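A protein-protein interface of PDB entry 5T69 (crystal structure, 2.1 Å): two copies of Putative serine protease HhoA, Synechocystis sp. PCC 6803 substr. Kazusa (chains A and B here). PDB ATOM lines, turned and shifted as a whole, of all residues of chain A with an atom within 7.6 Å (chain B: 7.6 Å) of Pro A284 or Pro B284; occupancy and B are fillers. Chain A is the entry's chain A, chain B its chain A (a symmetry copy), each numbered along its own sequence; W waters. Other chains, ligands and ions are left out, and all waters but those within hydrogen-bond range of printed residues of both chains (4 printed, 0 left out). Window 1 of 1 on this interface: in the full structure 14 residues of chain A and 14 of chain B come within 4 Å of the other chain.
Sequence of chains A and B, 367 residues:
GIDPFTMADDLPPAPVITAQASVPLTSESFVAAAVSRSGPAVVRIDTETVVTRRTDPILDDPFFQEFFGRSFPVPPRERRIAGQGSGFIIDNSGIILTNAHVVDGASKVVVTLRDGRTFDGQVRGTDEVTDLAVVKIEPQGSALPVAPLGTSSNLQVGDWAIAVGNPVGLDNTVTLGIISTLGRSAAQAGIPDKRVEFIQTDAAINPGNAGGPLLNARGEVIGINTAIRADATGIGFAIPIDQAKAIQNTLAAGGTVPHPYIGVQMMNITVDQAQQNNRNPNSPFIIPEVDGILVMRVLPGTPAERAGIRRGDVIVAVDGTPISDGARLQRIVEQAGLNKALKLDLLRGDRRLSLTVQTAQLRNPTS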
ATOM      1  N   ASN A 277       7.580  17.226   1.186  1.00  0.00           N
ATOM      2  CA  ASN A 277       6.709  16.302   1.907  1.00  0.00           C
ATOM      3  C   ASN A 277       7.501  15.124   2.420  1.00  0.00           C
ATOM      4  O   ASN A 277       7.442  14.783   3.610  1.00  0.00           O
ATOM      5  CB  ASN A 277       5.594  15.801   0.994  1.00  0.00           C
ATOM      6  CG  ASN A 277       4.726  14.749   1.668  1.00  0.00           C
ATOM      7  OD1 ASN A 277       3.780  15.099   2.339  1.00  0.00           O
ATOM      8  ND2 ASN A 277       5.046  13.462   1.498  1.00  0.00           N
ATOM      9  N   ASN A 280       9.531  15.326   5.603  1.00  0.00           N
ATOM     10  CA  ASN A 280       8.886  15.415   6.907  1.00  0.00           C
ATOM     11  C   ASN A 280       8.628  14.018   7.453  1.00  0.00           C
ATOM     12  O   ASN A 280       7.845  13.276   6.858  1.00  0.00           O
ATOM     13  CB  ASN A 280       7.582  16.200   6.769  1.00  0.00           C
ATOM     14  CG  ASN A 280       6.863  16.409   8.084  1.00  0.00           C
ATOM     15  OD1 ASN A 280       7.180  15.805   9.107  1.00  0.00           O
ATOM     16  ND2 ASN A 280       5.863  17.283   8.050  1.00  0.00           N
ATOM     17  N   PRO A 281       9.239  13.620   8.576  1.00  0.00           N
ATOM     18  CA  PRO A 281       9.016  12.256   9.080  1.00  0.00           C
ATOM     19  C   PRO A 281       7.564  11.956   9.349  1.00  0.00           C
ATOM     20  O   PRO A 281       7.178  10.778   9.376  1.00  0.00           O
ATOM     21  CB  PRO A 281       9.849  12.210  10.375  1.00  0.00           C
ATOM     22  CG  PRO A 281      10.830  13.251  10.247  1.00  0.00           C
ATOM     23  CD  PRO A 281      10.258  14.339   9.368  1.00  0.00           C
ATOM     24  N   ASN A 282       6.728  12.980   9.515  1.00  0.00           N
ATOM     25  CA  ASN A 282       5.337  12.778   9.911  1.00  0.00           C
ATOM     26  C   ASN A 282       4.337  13.059   8.796  1.00  0.00           C
ATOM     27  O   ASN A 282       3.136  13.066   9.058  1.00  0.00           O
ATOM     28  CB  ASN A 282       5.024  13.633  11.134  1.00  0.00           C
ATOM     29  CG  ASN A 282       5.699  13.100  12.364  1.00  0.00           C
ATOM     30  OD1 ASN A 282       5.538  11.911  12.707  1.00  0.00           O
ATOM     31  ND2 ASN A 282       6.532  13.946  13.006  1.00  0.00           N
ATOM     32  N   SER A 283       4.788  13.287   7.558  1.00  0.00           N
ATOM     33  CA  SER A 283       3.812  13.262   6.474  1.00  0.00           C
ATOM     34  C   SER A 283       3.105  11.902   6.474  1.00  0.00           C
ATOM     35  O   SER A 283       3.734  10.864   6.754  1.00  0.00           O
ATOM     36  CB  SER A 283       4.464  13.526   5.115  1.00  0.00           C
ATOM     37  OG  SER A 283       5.474  12.587   4.846  1.00  0.00           O
ATOM     38  N   PRO A 284       1.796  11.878   6.177  1.00  0.00           N
ATOM     39  CA  PRO A 284       1.071  10.600   6.184  1.00  0.00           C
ATOM     40  C   PRO A 284       1.614   9.605   5.174  1.00  0.00           C
ATOM     41  O   PRO A 284       1.599   8.399   5.446  1.00  0.00           O
ATOM     42  CB  PRO A 284      -0.372  11.012   5.870  1.00  0.00           C
ATOM     43  CG  PRO A 284      -0.261  12.279   5.142  1.00  0.00           C
ATOM     44  CD  PRO A 284       0.975  12.987   5.658  1.00  0.00           C
ATOM     45  N   PHE A 285       2.149  10.066   4.043  1.00  0.00           N
ATOM     46  CA  PHE A 285       2.606   9.127   3.031  1.00  0.00           C
ATOM     47  C   PHE A 285       3.696   9.752   2.176  1.00  0.00           C
ATOM     48  O   PHE A 285       3.745  10.971   2.009  1.00  0.00           O
ATOM     49  CB  PHE A 285       1.453   8.675   2.141  1.00  0.00           C
ATOM     50  CG  PHE A 285       0.615   9.797   1.631  1.00  0.00           C
ATOM     51  CD1 PHE A 285       1.037  10.553   0.552  1.00  0.00           C
ATOM     52  CD2 PHE A 285      -0.618  10.088   2.216  1.00  0.00           C
ATOM     53  CE1 PHE A 285       0.252  11.596   0.091  1.00  0.00           C
ATOM     54  CE2 PHE A 285      -1.398  11.140   1.748  1.00  0.00           C
ATOM     55  CZ  PHE A 285      -0.958  11.888   0.692  1.00  0.00           C
ATOM     56  N   ILE A 286       4.581   8.889   1.669  1.00  0.00           N
ATOM     57  CA  ILE A 286       5.610   9.288   0.710  1.00  0.00           C
ATOM     58  C   ILE A 286       4.960   9.544  -0.643  1.00  0.00           C
ATOM     59  O   ILE A 286       4.050   8.811  -1.059  1.00  0.00           O
ATOM     60  CB  ILE A 286       6.690   8.201   0.599  1.00  0.00           C
ATOM     61  CG1 ILE A 286       7.447   8.066   1.914  1.00  0.00           C
ATOM     62  CG2 ILE A 286       7.672   8.506  -0.537  1.00  0.00           C
ATOM     63  CD1 ILE A 286       8.300   6.803   1.987  1.00  0.00           C
ATOM     64  N   ILE A 287       5.425  10.579  -1.337  1.00  0.00           N
ATOM     65  CA  ILE A 287       4.856  11.016  -2.606  1.00  0.00           C
ATOM     66  C   ILE A 287       5.930  10.846  -3.674  1.00  0.00           C
ATOM     67  O   ILE A 287       7.066  11.257  -3.455  1.00  0.00           O
ATOM     68  CB  ILE A 287       4.390  12.481  -2.573  1.00  0.00           C
ATOM     69  CG1 ILE A 287       3.357  12.703  -1.489  1.00  0.00           C
ATOM     70  CG2 ILE A 287       3.827  12.910  -3.956  1.00  0.00           C
ATOM     71  CD1 ILE A 287       2.955  14.146  -1.337  1.00  0.00           C
ATOM     72  N   MET A 296      -6.108  13.727  -2.330  1.00  0.00           N
ATOM     73  CA  MET A 296      -6.099  14.053  -0.909  1.00  0.00           C
ATOM     74  C   MET A 296      -7.175  13.299  -0.174  1.00  0.00           C
ATOM     75  O   MET A 296      -7.006  12.962   1.003  1.00  0.00           O
ATOM     76  CB  MET A 296      -6.312  15.565  -0.677  1.00  0.00           C
ATOM     77  CG  MET A 296      -5.160  16.497  -1.132  1.00  0.00           C
ATOM     78  SD  MET A 296      -3.610  16.209  -0.228  1.00  0.00           S
ATOM     79  CE  MET A 296      -4.027  16.629   1.463  1.00  0.00           C
ATOM     80  N   ARG A 310      -7.225   5.404  -3.837  1.00  0.00           N
ATOM     81  CA  ARG A 310      -6.929   5.627  -2.427  1.00  0.00           C
ATOM     82  C   ARG A 310      -6.277   6.981  -2.221  1.00  0.00           C
ATOM     83  O   ARG A 310      -5.567   7.488  -3.098  1.00  0.00           O
ATOM     84  CB  ARG A 310      -5.972   4.575  -1.866  1.00  0.00           C
ATOM     85  CG  ARG A 310      -6.554   3.165  -1.721  1.00  0.00           C
ATOM     86  CD  ARG A 310      -5.423   2.250  -1.225  1.00  0.00           C
ATOM     87  NE  ARG A 310      -4.594   2.963  -0.246  1.00  0.00           N
ATOM     88  CZ  ARG A 310      -4.948   3.157   1.026  1.00  0.00           C
ATOM     89  NH1 ARG A 310      -6.110   2.685   1.477  1.00  0.00           N
ATOM     90  NH2 ARG A 310      -4.148   3.829   1.844  1.00  0.00           N
ATOM     91  N   ARG A 311      -6.498   7.535  -1.034  1.00  0.00           N
ATOM     92  CA  ARG A 311      -5.741   8.677  -0.564  1.00  0.00           C
ATOM     93  C   ARG A 311      -4.264   8.433  -0.753  1.00  0.00           C
ATOM     94  O   ARG A 311      -3.777   7.336  -0.491  1.00  0.00           O
ATOM     95  CB  ARG A 311      -6.033   8.903   0.914  1.00  0.00           C
ATOM     96  CG  ARG A 311      -5.085   9.918   1.615  1.00  0.00           C
ATOM     97  CD  ARG A 311      -5.494  10.023   3.101  1.00  0.00           C
ATOM     98  NE  ARG A 311      -4.826  11.132   3.796  1.00  0.00           N
ATOM     99  CZ  ARG A 311      -4.795  11.255   5.124  1.00  0.00           C
ATOM    100  NH1 ARG A 311      -5.408  10.340   5.891  1.00  0.00           N
ATOM    101  NH2 ARG A 311      -4.151  12.273   5.684  1.00  0.00           N
ATOM    102  N   GLY A 312      -3.554   9.464  -1.212  1.00  0.00           N
ATOM    103  CA  GLY A 312      -2.143   9.371  -1.488  1.00  0.00           C
ATOM    104  C   GLY A 312      -1.822   8.941  -2.895  1.00  0.00           C
ATOM    105  O   GLY A 312      -0.654   8.992  -3.288  1.00  0.00           O
ATOM    106  N   ASN B 277      -7.509  -1.364   8.316  1.00  0.00           N
ATOM    107  CA  ASN B 277      -6.918  -0.092   7.908  1.00  0.00           C
ATOM    108  C   ASN B 277      -6.821  -0.016   6.404  1.00  0.00           C
ATOM    109  O   ASN B 277      -7.271   0.956   5.782  1.00  0.00           O
ATOM    110  CB  ASN B 277      -5.526   0.065   8.512  1.00  0.00           C
ATOM    111  CG  ASN B 277      -4.825   1.325   8.026  1.00  0.00           C
ATOM    112  OD1 ASN B 277      -5.007   2.371   8.609  1.00  0.00           O
ATOM    113  ND2 ASN B 277      -4.031   1.232   6.954  1.00  0.00           N
ATOM    114  N   ASN B 280      -9.786   0.941   4.262  1.00  0.00           N
ATOM    115  CA  ASN B 280     -10.311   2.301   4.262  1.00  0.00           C
ATOM    116  C   ASN B 280      -9.594   3.130   3.205  1.00  0.00           C
ATOM    117  O   ASN B 280      -8.388   3.348   3.329  1.00  0.00           O
ATOM    118  CB  ASN B 280     -10.130   2.909   5.653  1.00  0.00           C
ATOM    119  CG  ASN B 280     -10.705   4.303   5.779  1.00  0.00           C
ATOM    120  OD1 ASN B 280     -11.062   4.955   4.799  1.00  0.00           O
ATOM    121  ND2 ASN B 280     -10.789   4.772   7.019  1.00  0.00           N
ATOM    122  N   PRO B 281     -10.283   3.624   2.169  1.00  0.00           N
ATOM    123  CA  PRO B 281      -9.580   4.394   1.131  1.00  0.00           C
ATOM    124  C   PRO B 281      -8.860   5.600   1.676  1.00  0.00           C
ATOM    125  O   PRO B 281      -7.921   6.093   1.034  1.00  0.00           O
ATOM    126  CB  PRO B 281     -10.705   4.803   0.162  1.00  0.00           C
ATOM    127  CG  PRO B 281     -11.775   3.872   0.388  1.00  0.00           C
ATOM    128  CD  PRO B 281     -11.701   3.401   1.822  1.00  0.00           C
ATOM    129  N   ASN B 282      -9.236   6.079   2.861  1.00  0.00           N
ATOM    130  CA  ASN B 282      -8.683   7.318   3.398  1.00  0.00           C
ATOM    131  C   ASN B 282      -7.739   7.107   4.575  1.00  0.00           C
ATOM    132  O   ASN B 282      -7.333   8.086   5.200  1.00  0.00           O
ATOM    133  CB  ASN B 282      -9.819   8.258   3.788  1.00  0.00           C
ATOM    134  CG  ASN B 282     -10.511   8.814   2.579  1.00  0.00           C
ATOM    135  OD1 ASN B 282      -9.858   9.392   1.687  1.00  0.00           O
ATOM    136  ND2 ASN B 282     -11.837   8.579   2.486  1.00  0.00           N
ATOM    137  N   SER B 283      -7.370   5.863   4.901  1.00  0.00           N
ATOM    138  CA  SER B 283      -6.255   5.716   5.830  1.00  0.00           C
ATOM    139  C   SER B 283      -5.030   6.434   5.253  1.00  0.00           C
ATOM    140  O   SER B 283      -4.810   6.420   4.027  1.00  0.00           O
ATOM    141  CB  SER B 283      -5.934   4.245   6.104  1.00  0.00           C
ATOM    142  OG  SER B 283      -5.634   3.562   4.914  1.00  0.00           O
ATOM    143  N   PRO B 284      -4.223   7.080   6.109  1.00  0.00           N
ATOM    144  CA  PRO B 284      -3.048   7.800   5.600  1.00  0.00           C
ATOM    145  C   PRO B 284      -2.055   6.891   4.899  1.00  0.00           C
ATOM    146  O   PRO B 284      -1.417   7.325   3.932  1.00  0.00           O
ATOM    147  CB  PRO B 284      -2.455   8.441   6.860  1.00  0.00           C
ATOM    148  CG  PRO B 284      -2.909   7.599   7.970  1.00  0.00           C
ATOM    149  CD  PRO B 284      -4.259   7.033   7.582  1.00  0.00           C
ATOM    150  N   PHE B 285      -1.941   5.627   5.307  1.00  0.00           N
ATOM    151  CA  PHE B 285      -0.943   4.763   4.699  1.00  0.00           C
ATOM    152  C   PHE B 285      -1.362   3.306   4.805  1.00  0.00           C
ATOM    153  O   PHE B 285      -2.086   2.924   5.725  1.00  0.00           O
ATOM    154  CB  PHE B 285       0.421   4.954   5.353  1.00  0.00           C
ATOM    155  CG  PHE B 285       0.380   4.921   6.843  1.00  0.00           C
ATOM    156  CD1 PHE B 285       0.321   3.714   7.516  1.00  0.00           C
ATOM    157  CD2 PHE B 285       0.423   6.104   7.583  1.00  0.00           C
ATOM    158  CE1 PHE B 285       0.278   3.697   8.900  1.00  0.00           C
ATOM    159  CE2 PHE B 285       0.376   6.076   8.972  1.00  0.00           C
ATOM    160  CZ  PHE B 285       0.301   4.877   9.622  1.00  0.00           C
ATOM    161  N   ILE B 286      -0.913   2.516   3.826  1.00  0.00           N
ATOM    162  CA  ILE B 286      -1.092   1.066   3.839  1.00  0.00           C
ATOM    163  C   ILE B 286      -0.155   0.455   4.873  1.00  0.00           C
ATOM    164  O   ILE B 286       0.998   0.885   5.018  1.00  0.00           O
ATOM    165  CB  ILE B 286      -0.821   0.479   2.446  1.00  0.00           C
ATOM    166  CG1 ILE B 286      -1.865   0.968   1.450  1.00  0.00           C
ATOM    167  CG2 ILE B 286      -0.813  -1.053   2.479  1.00  0.00           C
ATOM    168  CD1 ILE B 286      -1.480   0.698  -0.002  1.00  0.00           C
ATOM    169  N   ILE B 287      -0.645  -0.551   5.594  1.00  0.00           N
ATOM    170  CA  ILE B 287       0.084  -1.187   6.684  1.00  0.00           C
ATOM    171  C   ILE B 287       0.322  -2.641   6.292  1.00  0.00           C
ATOM    172  O   ILE B 287      -0.612  -3.303   5.847  1.00  0.00           O
ATOM    173  CB  ILE B 287      -0.677  -1.130   8.019  1.00  0.00           C
ATOM    174  CG1 ILE B 287      -0.977   0.298   8.419  1.00  0.00           C
ATOM    175  CG2 ILE B 287       0.122  -1.853   9.138  1.00  0.00           C
ATOM    176  CD1 ILE B 287      -1.824   0.403   9.658  1.00  0.00           C
ATOM    177  N   MET B 296       3.299   5.703  15.040  1.00  0.00           N
ATOM    178  CA  MET B 296       2.243   6.675  14.786  1.00  0.00           C
ATOM    179  C   MET B 296       2.810   8.059  14.618  1.00  0.00           C
ATOM    180  O   MET B 296       2.258   8.872  13.868  1.00  0.00           O
ATOM    181  CB  MET B 296       1.215   6.702  15.937  1.00  0.00           C
ATOM    182  CG  MET B 296       0.329   5.439  16.095  1.00  0.00           C
ATOM    183  SD  MET B 296      -0.744   5.137  14.660  1.00  0.00           S
ATOM    184  CE  MET B 296      -1.821   6.567  14.633  1.00  0.00           C
ATOM    185  N   ARG B 310      10.176   6.890  10.131  1.00  0.00           N
ATOM    186  CA  ARG B 310       9.059   7.685   9.636  1.00  0.00           C
ATOM    187  C   ARG B 310       7.741   7.154  10.171  1.00  0.00           C
ATOM    188  O   ARG B 310       7.593   5.953  10.423  1.00  0.00           O
ATOM    189  CB  ARG B 310       8.968   7.664   8.110  1.00  0.00           C
ATOM    190  CG  ARG B 310      10.081   8.415   7.373  1.00  0.00           C
ATOM    191  CD  ARG B 310       9.857   8.206   5.867  1.00  0.00           C
ATOM    192  NE  ARG B 310       8.422   8.245   5.563  1.00  0.00           N
ATOM    193  CZ  ARG B 310       7.711   9.370   5.478  1.00  0.00           C
ATOM    194  NH1 ARG B 310       8.302  10.551   5.665  1.00  0.00           N
ATOM    195  NH2 ARG B 310       6.411   9.318   5.218  1.00  0.00           N
ATOM    196  N   ARG B 311       6.782   8.064  10.299  1.00  0.00           N
ATOM    197  CA  ARG B 311       5.399   7.698  10.527  1.00  0.00           C
ATOM    198  C   ARG B 311       4.976   6.635   9.541  1.00  0.00           C
ATOM    199  O   ARG B 311       5.312   6.712   8.363  1.00  0.00           O
ATOM    200  CB  ARG B 311       4.516   8.927  10.357  1.00  0.00           C
ATOM    201  CG  ARG B 311       2.991   8.628  10.299  1.00  0.00           C
ATOM    202  CD  ARG B 311       2.238   9.963  10.109  1.00  0.00           C
ATOM    203  NE  ARG B 311       0.786   9.826  10.287  1.00  0.00           N
ATOM    204  CZ  ARG B 311      -0.093  10.752   9.903  1.00  0.00           C
ATOM    205  NH1 ARG B 311       0.343  11.886   9.334  1.00  0.00           N
ATOM    206  NH2 ARG B 311      -1.395  10.549  10.076  1.00  0.00           N
ATOM    207  N   GLY B 312       4.236   5.641  10.034  1.00  0.00           N
ATOM    208  CA  GLY B 312       3.797   4.531   9.228  1.00  0.00           C
ATOM    209  C   GLY B 312       4.758   3.372   9.206  1.00  0.00           C
ATOM    210  O   GLY B 312       4.407   2.309   8.689  1.00  0.00           O
HETATM  211  O   HOH W   1      10.507  11.535   6.147  1.00  0.00           O
HETATM  212  O   HOH W   2      -2.059   6.196   1.615  1.00  0.00           O
HETATM  213  O   HOH W   3       4.011   7.337   5.794  1.00  0.00           O
HETATM  214  O   HOH W   4      -8.078   1.406   0.729  1.00  0.00           O
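Water W1 lies within hydrogen-bond range of the guanidinium group (NH1) of Arg B310 (2.5 Å) and the backbone carbonyl oxygen (O) of Asn A280 (3.3 Å).
Water W4 lies within hydrogen-bond range of the guanidinium group (NH1) of Arg A310 (2.5 Å) and the backbone carbonyl oxygen (O) of Asn B280 (3.3 Å).
Water W2 lies within hydrogen-bond range of the backbone carbonyl oxygen (O) of Pro B284 (2.7 Å), the backbone carbonyl oxygen (O) of Arg A311 (2.9 Å) and the guanidinium group (NH2) of Arg A310 (3.2 Å).
Water W3 lies within hydrogen-bond range of O of Pro A284 (2.7 Å), O of Arg B311 (2.9 Å) and NH2 of Arg B310 (3.2 Å).
O of Pro A281 touches CA of Arg B310 (3.6 Å).
Ser A283 touches Arg B311 (O to CD, 3.8 Å).
Pro B284 touches Pro A284.
Phe B285 touches Pro A284.
O of Pro B284 touches CD2 of Phe A285, at 3.3 Å.
Arg B310 touches Ile A286 (NH2 to CG1, 3.7 Å).
Arg A310 touches Pro B281.
NH2 of Arg A310 touches CG1 of Ile B286, 3.7 Å away.
Ser B283 touches Arg A311 (O to CD, 3.8 Å).
Asn A277 touches none of the printed residues of chain B.
Of chain B, only Pro B284 (3.5 Å), Phe B285 (3.3 Å) and Arg B311 (3.5 Å) come within 4 Å of Pro A284.
Of the printed residues of chain A, Asn B280 touches Arg A310 (3.0 Å).
Of the printed residues of chain A, Pro B284 touches Pro A284 (3.5 Å), Phe A285 (3.3 Å) and Arg A311 (3.5 Å).
Of the printed residues of chain A, Phe B285 touches Pro A284.
Printed residues of chain A within 4 Å of Arg B311: Pro A281, Asn A282, Ser A283 and Pro A284.
The nearest residue of chain B that does not touch Pro A284 is Arg B310 (4.8 Å).
The side-chain amide nitrogen (ND2) of Asn B277 lies within hydrogen-bond range of the backbone carbonyl oxygen (O) of Phe B285 (2.9 Å).
The side-chain amide oxygen (OD1) of Asn B280 lies within hydrogen-bond range of the backbone NH (N) of Asn B282, 2.9 Å away.
The side-chain hydroxyl (OG) of Ser A283 lies within hydrogen-bond range of the backbone carbonyl oxygen (O) of Asn A280, 3.2 Å away.
The side-chain amide nitrogen (ND2) of Asn A277 lies within hydrogen-bond range of the backbone carbonyl oxygen (O) of Phe A285 (2.9 Å).
The backbone carbonyl oxygen of Asn B277 is in hydrogen-bond range of the side-chain hydroxyl of Ser B283, at 3.2 Å.
O of Asn A277 is in hydrogen-bond range of OG of Ser A283 (3.2 Å).
N of Pro B284 lies close to NH1 of Arg A311, 3.5 Å away.
NH1 of Arg B310 is in hydrogen-bond range of O of Asn A280.
NH2 of Arg A310 lies within hydrogen-bond range of OG of Ser B283.
The backbone NH of Arg A311 lies within hydrogen-bond range of the backbone carbonyl oxygen of Pro B281.
The guanidinium group (NH1) of Arg A310 is in hydrogen-bond range of the backbone carbonyl oxygen (O) of Asn B280 (3.0 Å).
The backbone carbonyl oxygen of Pro A281 lies within hydrogen-bond range of the backbone NH of Arg B311 (2.9 Å).
N of Pro A284 sits close to NH1 of Arg B311 (3.5 Å).
O of Asn B282 is in hydrogen-bond range of NH1 of Arg A311 (3.0 Å).
The backbone carbonyl oxygen (O) of Asn A282 lies within hydrogen-bond range of the guanidinium group (NH1) of Arg B311, 3.0 Å away.
OG of Ser A283 is in hydrogen-bond range of NH2 of Arg B310 (3.4 Å).
Of the 13 printed residues of chain A, 9 touch a printed residue of chain B.
Printed residues of chain B that touch a printed residue of chain A: Asn B280, Pro B281, Asn B282, Ser B283, Pro B284, Phe B285, Ile B286, Arg B310 and Arg B311.
Along chain B the printed residues that touch a printed residue of chain A span positions 280 to 311.
Among the printed residues, 19 pairs touch across the chains.
Among the printed residues, no Asp or Glu carboxylate lies within 4 Å of a Lys or Arg side-chain nitrogen of the other chain.
Pro A281 touches Arg B311, and with the chains exchanged Arg A311 touches Pro B281.
Asn A282 touches Arg B311, and with the chains exchanged Arg A311 touches Asn B282.
Ser A283 touches Arg B311, and with the chains exchanged Arg A311 touches Ser B283.
Ile A286 touches Arg B310, and with the chains exchanged Arg A310 touches Ile B286.
Positions printed for both chains: 277, 280, 281, 282, 283, 284, 285, 286, 287, 296, 310, 311 and 312.
Of the 19 pairs that touch across the chains among the printed residues, 19 have their exchanged pair printed and touching as well.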
